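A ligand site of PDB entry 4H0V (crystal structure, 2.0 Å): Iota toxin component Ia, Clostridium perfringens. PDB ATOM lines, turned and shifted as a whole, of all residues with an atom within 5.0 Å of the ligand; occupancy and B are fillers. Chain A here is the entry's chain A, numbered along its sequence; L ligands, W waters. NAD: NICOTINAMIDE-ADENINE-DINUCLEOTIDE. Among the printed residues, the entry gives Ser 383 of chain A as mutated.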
ATOM      1  N   TYR A 256      -1.962  13.436  39.691  1.00  0.00           N
ATOM      2  CA  TYR A 256      -1.590  13.348  38.279  1.00  0.00           C
ATOM      3  C   TYR A 256      -0.298  14.074  37.976  1.00  0.00           C
ATOM      4  O   TYR A 256       0.492  13.602  37.166  1.00  0.00           O
ATOM      5  CB  TYR A 256      -2.721  13.799  37.335  1.00  0.00           C
ATOM      6  CG  TYR A 256      -3.179  15.252  37.383  1.00  0.00           C
ATOM      7  CD1 TYR A 256      -4.378  15.592  37.992  1.00  0.00           C
ATOM      8  CD2 TYR A 256      -2.456  16.257  36.745  1.00  0.00           C
ATOM      9  CE1 TYR A 256      -4.823  16.900  38.017  1.00  0.00           C
ATOM     10  CE2 TYR A 256      -2.897  17.578  36.765  1.00  0.00           C
ATOM     11  CZ  TYR A 256      -4.088  17.885  37.397  1.00  0.00           C
ATOM     12  OH  TYR A 256      -4.537  19.190  37.430  1.00  0.00           O
ATOM     13  N   ASN A 260       2.473  11.959  36.293  1.00  0.00           N
ATOM     14  CA  ASN A 260       2.755  12.284  34.901  1.00  0.00           C
ATOM     15  C   ASN A 260       4.158  12.841  34.692  1.00  0.00           C
ATOM     16  O   ASN A 260       4.786  12.546  33.680  1.00  0.00           O
ATOM     17  CB  ASN A 260       1.687  13.222  34.332  1.00  0.00           C
ATOM     18  CG  ASN A 260       0.351  12.527  34.089  1.00  0.00           C
ATOM     19  OD1 ASN A 260       0.292  11.310  33.892  1.00  0.00           O
ATOM     20  ND2 ASN A 260      -0.727  13.294  34.088  1.00  0.00           N
ATOM     21  N   ILE A 264       6.923  11.369  32.179  1.00  0.00           N
ATOM     22  CA  ILE A 264       7.532  12.225  31.155  1.00  0.00           C
ATOM     23  C   ILE A 264       9.059  12.314  31.308  1.00  0.00           C
ATOM     24  O   ILE A 264       9.778  12.353  30.303  1.00  0.00           O
ATOM     25  CB  ILE A 264       6.907  13.645  31.172  1.00  0.00           C
ATOM     26  CG1 ILE A 264       5.435  13.564  30.731  1.00  0.00           C
ATOM     27  CG2 ILE A 264       7.674  14.610  30.255  1.00  0.00           C
ATOM     28  CD1 ILE A 264       4.654  14.847  30.942  1.00  0.00           C
ATOM     29  N   TYR A 299     -12.238  15.923  23.043  1.00  0.00           N
ATOM     30  CA  TYR A 299     -11.644  17.237  22.850  1.00  0.00           C
ATOM     31  C   TYR A 299     -10.713  17.545  24.006  1.00  0.00           C
ATOM     32  O   TYR A 299     -11.018  17.230  25.162  1.00  0.00           O
ATOM     33  CB  TYR A 299     -12.763  18.283  22.771  1.00  0.00           C
ATOM     34  CG  TYR A 299     -13.703  18.072  21.596  1.00  0.00           C
ATOM     35  CD1 TYR A 299     -14.750  17.146  21.662  1.00  0.00           C
ATOM     36  CD2 TYR A 299     -13.529  18.780  20.413  1.00  0.00           C
ATOM     37  CE1 TYR A 299     -15.599  16.951  20.586  1.00  0.00           C
ATOM     38  CE2 TYR A 299     -14.375  18.589  19.328  1.00  0.00           C
ATOM     39  CZ  TYR A 299     -15.405  17.674  19.416  1.00  0.00           C
ATOM     40  OH  TYR A 299     -16.242  17.490  18.339  1.00  0.00           O
ATOM     41  N   ARG A 300      -9.559  18.128  23.692  1.00  0.00           N
ATOM     42  CA  ARG A 300      -8.623  18.579  24.705  1.00  0.00           C
ATOM     43  C   ARG A 300      -8.110  19.951  24.322  1.00  0.00           C
ATOM     44  O   ARG A 300      -7.663  20.167  23.199  1.00  0.00           O
ATOM     45  CB  ARG A 300      -7.446  17.609  24.851  1.00  0.00           C
ATOM     46  CG  ARG A 300      -6.224  18.201  25.525  1.00  0.00           C
ATOM     47  CD  ARG A 300      -5.119  17.182  25.738  1.00  0.00           C
ATOM     48  NE  ARG A 300      -4.037  17.823  26.485  1.00  0.00           N
ATOM     49  CZ  ARG A 300      -4.022  18.006  27.795  1.00  0.00           C
ATOM     50  NH1 ARG A 300      -5.013  17.554  28.574  1.00  0.00           N
ATOM     51  NH2 ARG A 300      -2.996  18.632  28.364  1.00  0.00           N
ATOM     52  N   ARG A 301      -8.186  20.859  25.280  1.00  0.00           N
ATOM     53  CA  ARG A 301      -7.594  22.161  25.162  1.00  0.00           C
ATOM     54  C   ARG A 301      -6.157  22.073  25.688  1.00  0.00           C
ATOM     55  O   ARG A 301      -5.927  21.985  26.892  1.00  0.00           O
ATOM     56  CB  ARG A 301      -8.434  23.156  25.963  1.00  0.00           C
ATOM     57  CG  ARG A 301      -9.359  24.008  25.109  1.00  0.00           C
ATOM     58  CD  ARG A 301     -10.835  23.662  24.840  1.00  0.00           C
ATOM     59  NE  ARG A 301     -11.162  24.975  24.287  1.00  0.00           N
ATOM     60  CZ  ARG A 301     -12.141  25.447  23.524  1.00  0.00           C
ATOM     61  NH1 ARG A 301     -13.286  24.814  23.173  1.00  0.00           N
ATOM     62  NH2 ARG A 301     -11.973  26.729  23.179  1.00  0.00           N
ATOM     63  N   SER A 302      -5.202  22.078  24.757  1.00  0.00           N
ATOM     64  CA  SER A 302      -3.784  21.858  25.091  1.00  0.00           C
ATOM     65  C   SER A 302      -3.079  23.117  25.562  1.00  0.00           C
ATOM     66  O   SER A 302      -3.342  24.209  25.052  1.00  0.00           O
ATOM     67  CB  SER A 302      -3.029  21.327  23.861  1.00  0.00           C
ATOM     68  OG  SER A 302      -3.354  19.969  23.617  1.00  0.00           O
ATOM     69  N   GLY A 303      -2.177  22.954  26.524  1.00  0.00           N
ATOM     70  CA  GLY A 303      -1.223  24.004  26.848  1.00  0.00           C
ATOM     71  C   GLY A 303      -0.221  24.102  25.709  1.00  0.00           C
ATOM     72  O   GLY A 303       0.040  23.100  25.033  1.00  0.00           O
ATOM     73  N   PRO A 304       0.343  25.303  25.478  1.00  0.00           N
ATOM     74  CA  PRO A 304       1.286  25.412  24.368  1.00  0.00           C
ATOM     75  C   PRO A 304       2.550  24.549  24.536  1.00  0.00           C
ATOM     76  O   PRO A 304       3.213  24.254  23.547  1.00  0.00           O
ATOM     77  CB  PRO A 304       1.658  26.898  24.351  1.00  0.00           C
ATOM     78  CG  PRO A 304       1.289  27.413  25.697  1.00  0.00           C
ATOM     79  CD  PRO A 304       0.139  26.581  26.169  1.00  0.00           C
ATOM     80  N   GLN A 305       2.862  24.147  25.771  1.00  0.00           N
ATOM     81  CA  GLN A 305       4.081  23.390  26.049  1.00  0.00           C
ATOM     82  C   GLN A 305       4.049  22.002  25.406  1.00  0.00           C
ATOM     83  O   GLN A 305       5.095  21.418  25.128  1.00  0.00           O
ATOM     84  CB  GLN A 305       4.357  23.285  27.551  1.00  0.00           C
ATOM     85  CG  GLN A 305       4.596  24.639  28.224  1.00  0.00           C
ATOM     86  CD  GLN A 305       3.320  25.333  28.670  1.00  0.00           C
ATOM     87  OE1 GLN A 305       2.207  24.842  28.439  1.00  0.00           O
ATOM     88  NE2 GLN A 305       3.458  26.487  29.309  1.00  0.00           N
ATOM     89  N   GLU A 306       2.850  21.477  25.162  1.00  0.00           N
ATOM     90  CA  GLU A 306       2.687  20.199  24.459  1.00  0.00           C
ATOM     91  C   GLU A 306       3.197  20.257  23.025  1.00  0.00           C
ATOM     92  O   GLU A 306       3.553  19.229  22.443  1.00  0.00           O
ATOM     93  CB  GLU A 306       1.219  19.792  24.444  1.00  0.00           C
ATOM     94  CG  GLU A 306       0.748  19.279  25.785  1.00  0.00           C
ATOM     95  CD  GLU A 306      -0.749  19.390  25.939  1.00  0.00           C
ATOM     96  OE1 GLU A 306      -1.480  18.750  25.152  1.00  0.00           O
ATOM     97  OE2 GLU A 306      -1.208  20.106  26.854  1.00  0.00           O
ATOM     98  N   THR A 337       3.457  11.609  20.707  1.00  0.00           N
ATOM     99  CA  THR A 337       3.244  10.684  21.816  1.00  0.00           C
ATOM    100  C   THR A 337       3.239  11.412  23.138  1.00  0.00           C
ATOM    101  O   THR A 337       4.016  12.348  23.345  1.00  0.00           O
ATOM    102  CB  THR A 337       4.364   9.643  21.932  1.00  0.00           C
ATOM    103  OG1 THR A 337       4.948   9.403  20.637  1.00  0.00           O
ATOM    104  CG2 THR A 337       3.824   8.356  22.493  1.00  0.00           C
ATOM    105  N   TYR A 338       2.396  10.940  24.045  1.00  0.00           N
ATOM    106  CA  TYR A 338       2.294  11.473  25.395  1.00  0.00           C
ATOM    107  C   TYR A 338       2.757  10.382  26.339  1.00  0.00           C
ATOM    108  O   TYR A 338       2.064   9.372  26.479  1.00  0.00           O
ATOM    109  CB  TYR A 338       0.844  11.855  25.698  1.00  0.00           C
ATOM    110  CG  TYR A 338       0.423  13.176  25.113  1.00  0.00           C
ATOM    111  CD1 TYR A 338       0.356  14.316  25.900  1.00  0.00           C
ATOM    112  CD2 TYR A 338       0.091  13.280  23.763  1.00  0.00           C
ATOM    113  CE1 TYR A 338      -0.034  15.537  25.363  1.00  0.00           C
ATOM    114  CE2 TYR A 338      -0.296  14.495  23.214  1.00  0.00           C
ATOM    115  CZ  TYR A 338      -0.361  15.617  24.016  1.00  0.00           C
ATOM    116  OH  TYR A 338      -0.742  16.827  23.478  1.00  0.00           O
ATOM    117  N   PRO A 339       3.922  10.560  26.984  1.00  0.00           N
ATOM    118  CA  PRO A 339       4.287   9.548  27.983  1.00  0.00           C
ATOM    119  C   PRO A 339       3.331   9.547  29.170  1.00  0.00           C
ATOM    120  O   PRO A 339       3.151   8.522  29.820  1.00  0.00           O
ATOM    121  CB  PRO A 339       5.704   9.944  28.414  1.00  0.00           C
ATOM    122  CG  PRO A 339       6.158  11.003  27.467  1.00  0.00           C
ATOM    123  CD  PRO A 339       4.941  11.604  26.833  1.00  0.00           C
ATOM    124  N   ASN A 340       2.741  10.704  29.444  1.00  0.00           N
ATOM    125  CA  ASN A 340       1.733  10.852  30.503  1.00  0.00           C
ATOM    126  C   ASN A 340       0.355  10.313  30.140  1.00  0.00           C
ATOM    127  O   ASN A 340       0.010  10.227  28.967  1.00  0.00           O
ATOM    128  CB  ASN A 340       1.596  12.323  30.911  1.00  0.00           C
ATOM    129  CG  ASN A 340       1.499  13.286  29.726  1.00  0.00           C
ATOM    130  OD1 ASN A 340       2.184  13.122  28.711  1.00  0.00           O
ATOM    131  ND2 ASN A 340       0.649  14.299  29.861  1.00  0.00           N
ATOM    132  N   SER A 343      -5.810  13.860  29.762  1.00  0.00           N
ATOM    133  CA  SER A 343      -7.209  14.185  29.966  1.00  0.00           C
ATOM    134  C   SER A 343      -7.841  14.775  28.715  1.00  0.00           C
ATOM    135  O   SER A 343      -7.246  15.622  28.052  1.00  0.00           O
ATOM    136  CB  SER A 343      -7.370  15.204  31.103  1.00  0.00           C
ATOM    137  OG  SER A 343      -7.067  14.607  32.353  1.00  0.00           O
ATOM    138  N   THR A 344      -9.048  14.315  28.428  1.00  0.00           N
ATOM    139  CA  THR A 344      -9.859  14.854  27.354  1.00  0.00           C
ATOM    140  C   THR A 344     -11.291  14.950  27.849  1.00  0.00           C
ATOM    141  O   THR A 344     -11.620  14.406  28.907  1.00  0.00           O
ATOM    142  CB  THR A 344      -9.823  13.949  26.104  1.00  0.00           C
ATOM    143  OG1 THR A 344     -10.495  12.715  26.395  1.00  0.00           O
ATOM    144  CG2 THR A 344      -8.402  13.648  25.699  1.00  0.00           C
ATOM    145  N   SER A 345     -12.137  15.624  27.086  1.00  0.00           N
ATOM    146  CA  SER A 345     -13.555  15.718  27.390  1.00  0.00           C
ATOM    147  C   SER A 345     -14.418  15.247  26.222  1.00  0.00           C
ATOM    148  O   SER A 345     -14.005  15.328  25.062  1.00  0.00           O
ATOM    149  CB  SER A 345     -13.935  17.165  27.707  1.00  0.00           C
ATOM    150  OG  SER A 345     -15.320  17.298  27.994  1.00  0.00           O
ATOM    151  N   PHE A 354      -9.759  26.969  30.958  1.00  0.00           N
ATOM    152  CA  PHE A 354      -8.858  27.058  29.800  1.00  0.00           C
ATOM    153  C   PHE A 354      -9.390  27.922  28.662  1.00  0.00           C
ATOM    154  O   PHE A 354      -9.160  27.659  27.478  1.00  0.00           O
ATOM    155  CB  PHE A 354      -8.461  25.665  29.316  1.00  0.00           C
ATOM    156  CG  PHE A 354      -9.597  24.719  29.097  1.00  0.00           C
ATOM    157  CD1 PHE A 354     -10.653  25.035  28.248  1.00  0.00           C
ATOM    158  CD2 PHE A 354      -9.581  23.474  29.701  1.00  0.00           C
ATOM    159  CE1 PHE A 354     -11.672  24.149  28.030  1.00  0.00           C
ATOM    160  CE2 PHE A 354     -10.603  22.575  29.487  1.00  0.00           C
ATOM    161  CZ  PHE A 354     -11.649  22.908  28.650  1.00  0.00           C
ATOM    162  N   ARG A 357      -6.685  29.055  26.066  1.00  0.00           N
ATOM    163  CA  ARG A 357      -5.838  28.083  25.359  1.00  0.00           C
ATOM    164  C   ARG A 357      -6.163  28.070  23.879  1.00  0.00           C
ATOM    165  O   ARG A 357      -7.335  28.056  23.500  1.00  0.00           O
ATOM    166  CB  ARG A 357      -6.012  26.683  25.938  1.00  0.00           C
ATOM    167  CG  ARG A 357      -5.265  26.514  27.243  1.00  0.00           C
ATOM    168  CD  ARG A 357      -5.255  25.086  27.719  1.00  0.00           C
ATOM    169  NE  ARG A 357      -4.334  24.945  28.848  1.00  0.00           N
ATOM    170  CZ  ARG A 357      -4.134  23.840  29.559  1.00  0.00           C
ATOM    171  NH1 ARG A 357      -4.790  22.717  29.293  1.00  0.00           N
ATOM    172  NH2 ARG A 357      -3.264  23.857  30.565  1.00  0.00           N
ATOM    173  N   SER A 383     -15.908  17.949  34.584  1.00  0.00           N
ATOM    174  CA  SER A 383     -14.955  17.865  33.463  1.00  0.00           C
ATOM    175  C   SER A 383     -15.532  17.198  32.214  1.00  0.00           C
ATOM    176  O   SER A 383     -15.061  17.451  31.104  1.00  0.00           O
ATOM    177  CB  SER A 383     -13.697  17.103  33.893  1.00  0.00           C
ATOM    178  OG  SER A 383     -12.932  17.858  34.812  1.00  0.00           O
ATOM    179  N   GLU A 385     -15.026  14.059  31.710  1.00  0.00           N
ATOM    180  CA  GLU A 385     -13.673  13.626  31.384  1.00  0.00           C
ATOM    181  C   GLU A 385     -13.569  12.192  30.898  1.00  0.00           C
ATOM    182  O   GLU A 385     -14.178  11.283  31.460  1.00  0.00           O
ATOM    183  CB  GLU A 385     -12.766  13.826  32.587  1.00  0.00           C
ATOM    184  CG  GLU A 385     -11.294  13.504  32.320  1.00  0.00           C
ATOM    185  CD  GLU A 385     -10.418  13.769  33.529  1.00  0.00           C
ATOM    186  OE1 GLU A 385      -9.182  13.698  33.386  1.00  0.00           O
ATOM    187  OE2 GLU A 385     -10.964  14.058  34.616  1.00  0.00           O
HETATM  188  PA  NAD L   1      -2.000  18.699  32.188  1.00  0.00           P
HETATM  189  O1A NAD L   1      -1.501  18.035  33.448  1.00  0.00           O
HETATM  190  O2A NAD L   1      -2.381  17.886  30.972  1.00  0.00           O
HETATM  191  O5B NAD L   1      -0.936  19.802  31.710  1.00  0.00           O
HETATM  192  C5B NAD L   1      -0.098  20.497  32.631  1.00  0.00           C
HETATM  193  C4B NAD L   1       0.954  21.233  31.826  1.00  0.00           C
HETATM  194  O4B NAD L   1       1.845  20.282  31.236  1.00  0.00           O
HETATM  195  C3B NAD L   1       0.388  22.025  30.654  1.00  0.00           C
HETATM  196  O3B NAD L   1       1.200  23.184  30.417  1.00  0.00           O
HETATM  197  C2B NAD L   1       0.483  21.078  29.466  1.00  0.00           C
HETATM  198  O2B NAD L   1       0.598  21.773  28.220  1.00  0.00           O
HETATM  199  C1B NAD L   1       1.773  20.354  29.809  1.00  0.00           C
HETATM  200  N9A NAD L   1       1.924  18.992  29.280  1.00  0.00           N
HETATM  201  C8A NAD L   1       1.116  17.923  29.489  1.00  0.00           C
HETATM  202  N7A NAD L   1       1.620  16.831  28.865  1.00  0.00           N
HETATM  203  C5A NAD L   1       2.758  17.198  28.254  1.00  0.00           C
HETATM  204  C6A NAD L   1       3.787  16.541  27.418  1.00  0.00           C
HETATM  205  N6A NAD L   1       3.666  15.230  27.121  1.00  0.00           N
HETATM  206  N1A NAD L   1       4.826  17.294  26.985  1.00  0.00           N
HETATM  207  C2A NAD L   1       4.956  18.603  27.284  1.00  0.00           C
HETATM  208  N3A NAD L   1       4.057  19.258  28.041  1.00  0.00           N
HETATM  209  C4A NAD L   1       2.966  18.620  28.540  1.00  0.00           C
HETATM  210  O3  NAD L   1      -3.176  19.679  32.648  1.00  0.00           O
HETATM  211  PN  NAD L   1      -4.613  19.792  31.924  1.00  0.00           P
HETATM  212  O1N NAD L   1      -4.938  18.525  31.165  1.00  0.00           O
HETATM  213  O2N NAD L   1      -4.691  21.170  31.251  1.00  0.00           O
HETATM  214  O5D NAD L   1      -5.503  19.912  33.247  1.00  0.00           O
HETATM  215  C5D NAD L   1      -5.925  18.709  33.854  1.00  0.00           C
HETATM  216  C4D NAD L   1      -7.081  19.105  34.747  1.00  0.00           C
HETATM  217  O4D NAD L   1      -8.151  19.607  33.951  1.00  0.00           O
HETATM  218  C3D NAD L   1      -7.567  17.819  35.375  1.00  0.00           C
HETATM  219  O3D NAD L   1      -8.311  18.105  36.560  1.00  0.00           O
HETATM  220  C2D NAD L   1      -8.463  17.273  34.277  1.00  0.00           C
HETATM  221  O2D NAD L   1      -9.476  16.402  34.796  1.00  0.00           O
HETATM  222  C1D NAD L   1      -9.071  18.533  33.676  1.00  0.00           C
HETATM  223  N1N NAD L   1      -9.389  18.401  32.239  1.00  0.00           N
HETATM  224  C2N NAD L   1      -8.733  19.094  31.278  1.00  0.00           C
HETATM  225  C3N NAD L   1      -9.075  18.959  29.922  1.00  0.00           C
HETATM  226  C7N NAD L   1      -8.376  19.715  28.819  1.00  0.00           C
HETATM  227  O7N NAD L   1      -8.937  19.826  27.744  1.00  0.00           O
HETATM  228  N7N NAD L   1      -7.178  20.294  28.994  1.00  0.00           N
HETATM  229  C4N NAD L   1     -10.110  18.083  29.587  1.00  0.00           C
HETATM  230  C5N NAD L   1     -10.769  17.391  30.594  1.00  0.00           C
HETATM  231  C6N NAD L   1     -10.387  17.573  31.916  1.00  0.00           C
HETATM  232  O   HOH W   1       7.470  16.139  26.251  1.00  0.00           O
HETATM  233  O   HOH W   2       0.202  18.823  35.834  1.00  0.00           O
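The guanidinium group of Arg 357 is in salt-bridge range of an oxygen (O2N) of the ligand, at 2.5 Å. NH1 of Arg 300 lies within salt-bridge range of O1N of the ligand (2.8 Å). The side-chain amide oxygen (OE1) of Gln 305 is in hydrogen-bond range of an oxygen (O3B) of the ligand (2.8 Å). An oxygen (O7N) of the ligand lies within hydrogen-bond range of the backbone NH of Arg 301 (2.8 Å). O of Arg 301 lies within hydrogen-bond range of N7N of the ligand, at 3.0 Å. The side-chain carboxylate (OE2) of Glu 385 lies within hydrogen-bond range of an oxygen (O2D) of the ligand. O2B of the ligand sits at hydrogen-bond distance from OE2 of Glu 306, at 2.8 Å. A nitrogen (N7A) of the ligand lies within hydrogen-bond range of the side-chain amide nitrogen (ND2) of Asn 340 (2.9 Å). An oxygen (O2B) of the ligand lies close to the backbone NH (N) of Gly 303 (3.5 Å). The backbone carbonyl oxygen (O) of Gly 303 sits close to an oxygen (O2B) of the ligand, at 3.5 Å.
Tyr 256 touches the ligand (CE2 to O1A, 3.6 Å). CD1 of Ile 264 touches N6A of the ligand (3.97 Å). Tyr 338 touches the ligand (CD1 to N6A, 3.6 Å). Pro 339 touches the ligand (CD to N6A, 3.9 Å). Ser 343 touches the ligand. O of Thr 344 touches C5N of the ligand, 3.5 Å away. Phe 354 touches the ligand. Ser 383 touches the ligand (OG to O2D, 3.8 Å). Hydrophobic or aromatic side chains within 4 Å of the ligand: Tyr 256, Ile 264, Tyr 338, Pro 339 and Phe 354. Of the 22 residues printed, 16 come within 4 Å of the ligand.
NH1 of Arg 357 lies within hydrogen-bond range of O of Arg 301, at 2.8 Å. The guanidinium group (NH1) of Arg 300 lies within hydrogen-bond range of the backbone carbonyl oxygen (O) of Ser 343, at 3.0 Å. The side-chain carboxylate (OE1) of Glu 385 lies within hydrogen-bond range of the side-chain hydroxyl (OG) of Ser 343, 2.5 Å away. The backbone NH of Gly 303 lies within hydrogen-bond range of the side-chain carboxylate of Glu 306 (3.0 Å). The side-chain hydroxyl (OH) of Tyr 338 sits at hydrogen-bond distance from the side-chain carboxylate (OE1) of Glu 306 (2.7 Å). The side-chain carboxylate (OE1) of Glu 306 sits at hydrogen-bond distance from the side-chain hydroxyl (OG) of Ser 302, 2.7 Å away. The backbone carbonyl oxygen of Tyr 256 sits close to the side-chain amide nitrogen of Asn 260, 3.3 Å away. The backbone carbonyl oxygen of Ser 383 lies within hydrogen-bond range of the side-chain hydroxyl of Ser 345, 3.1 Å away.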
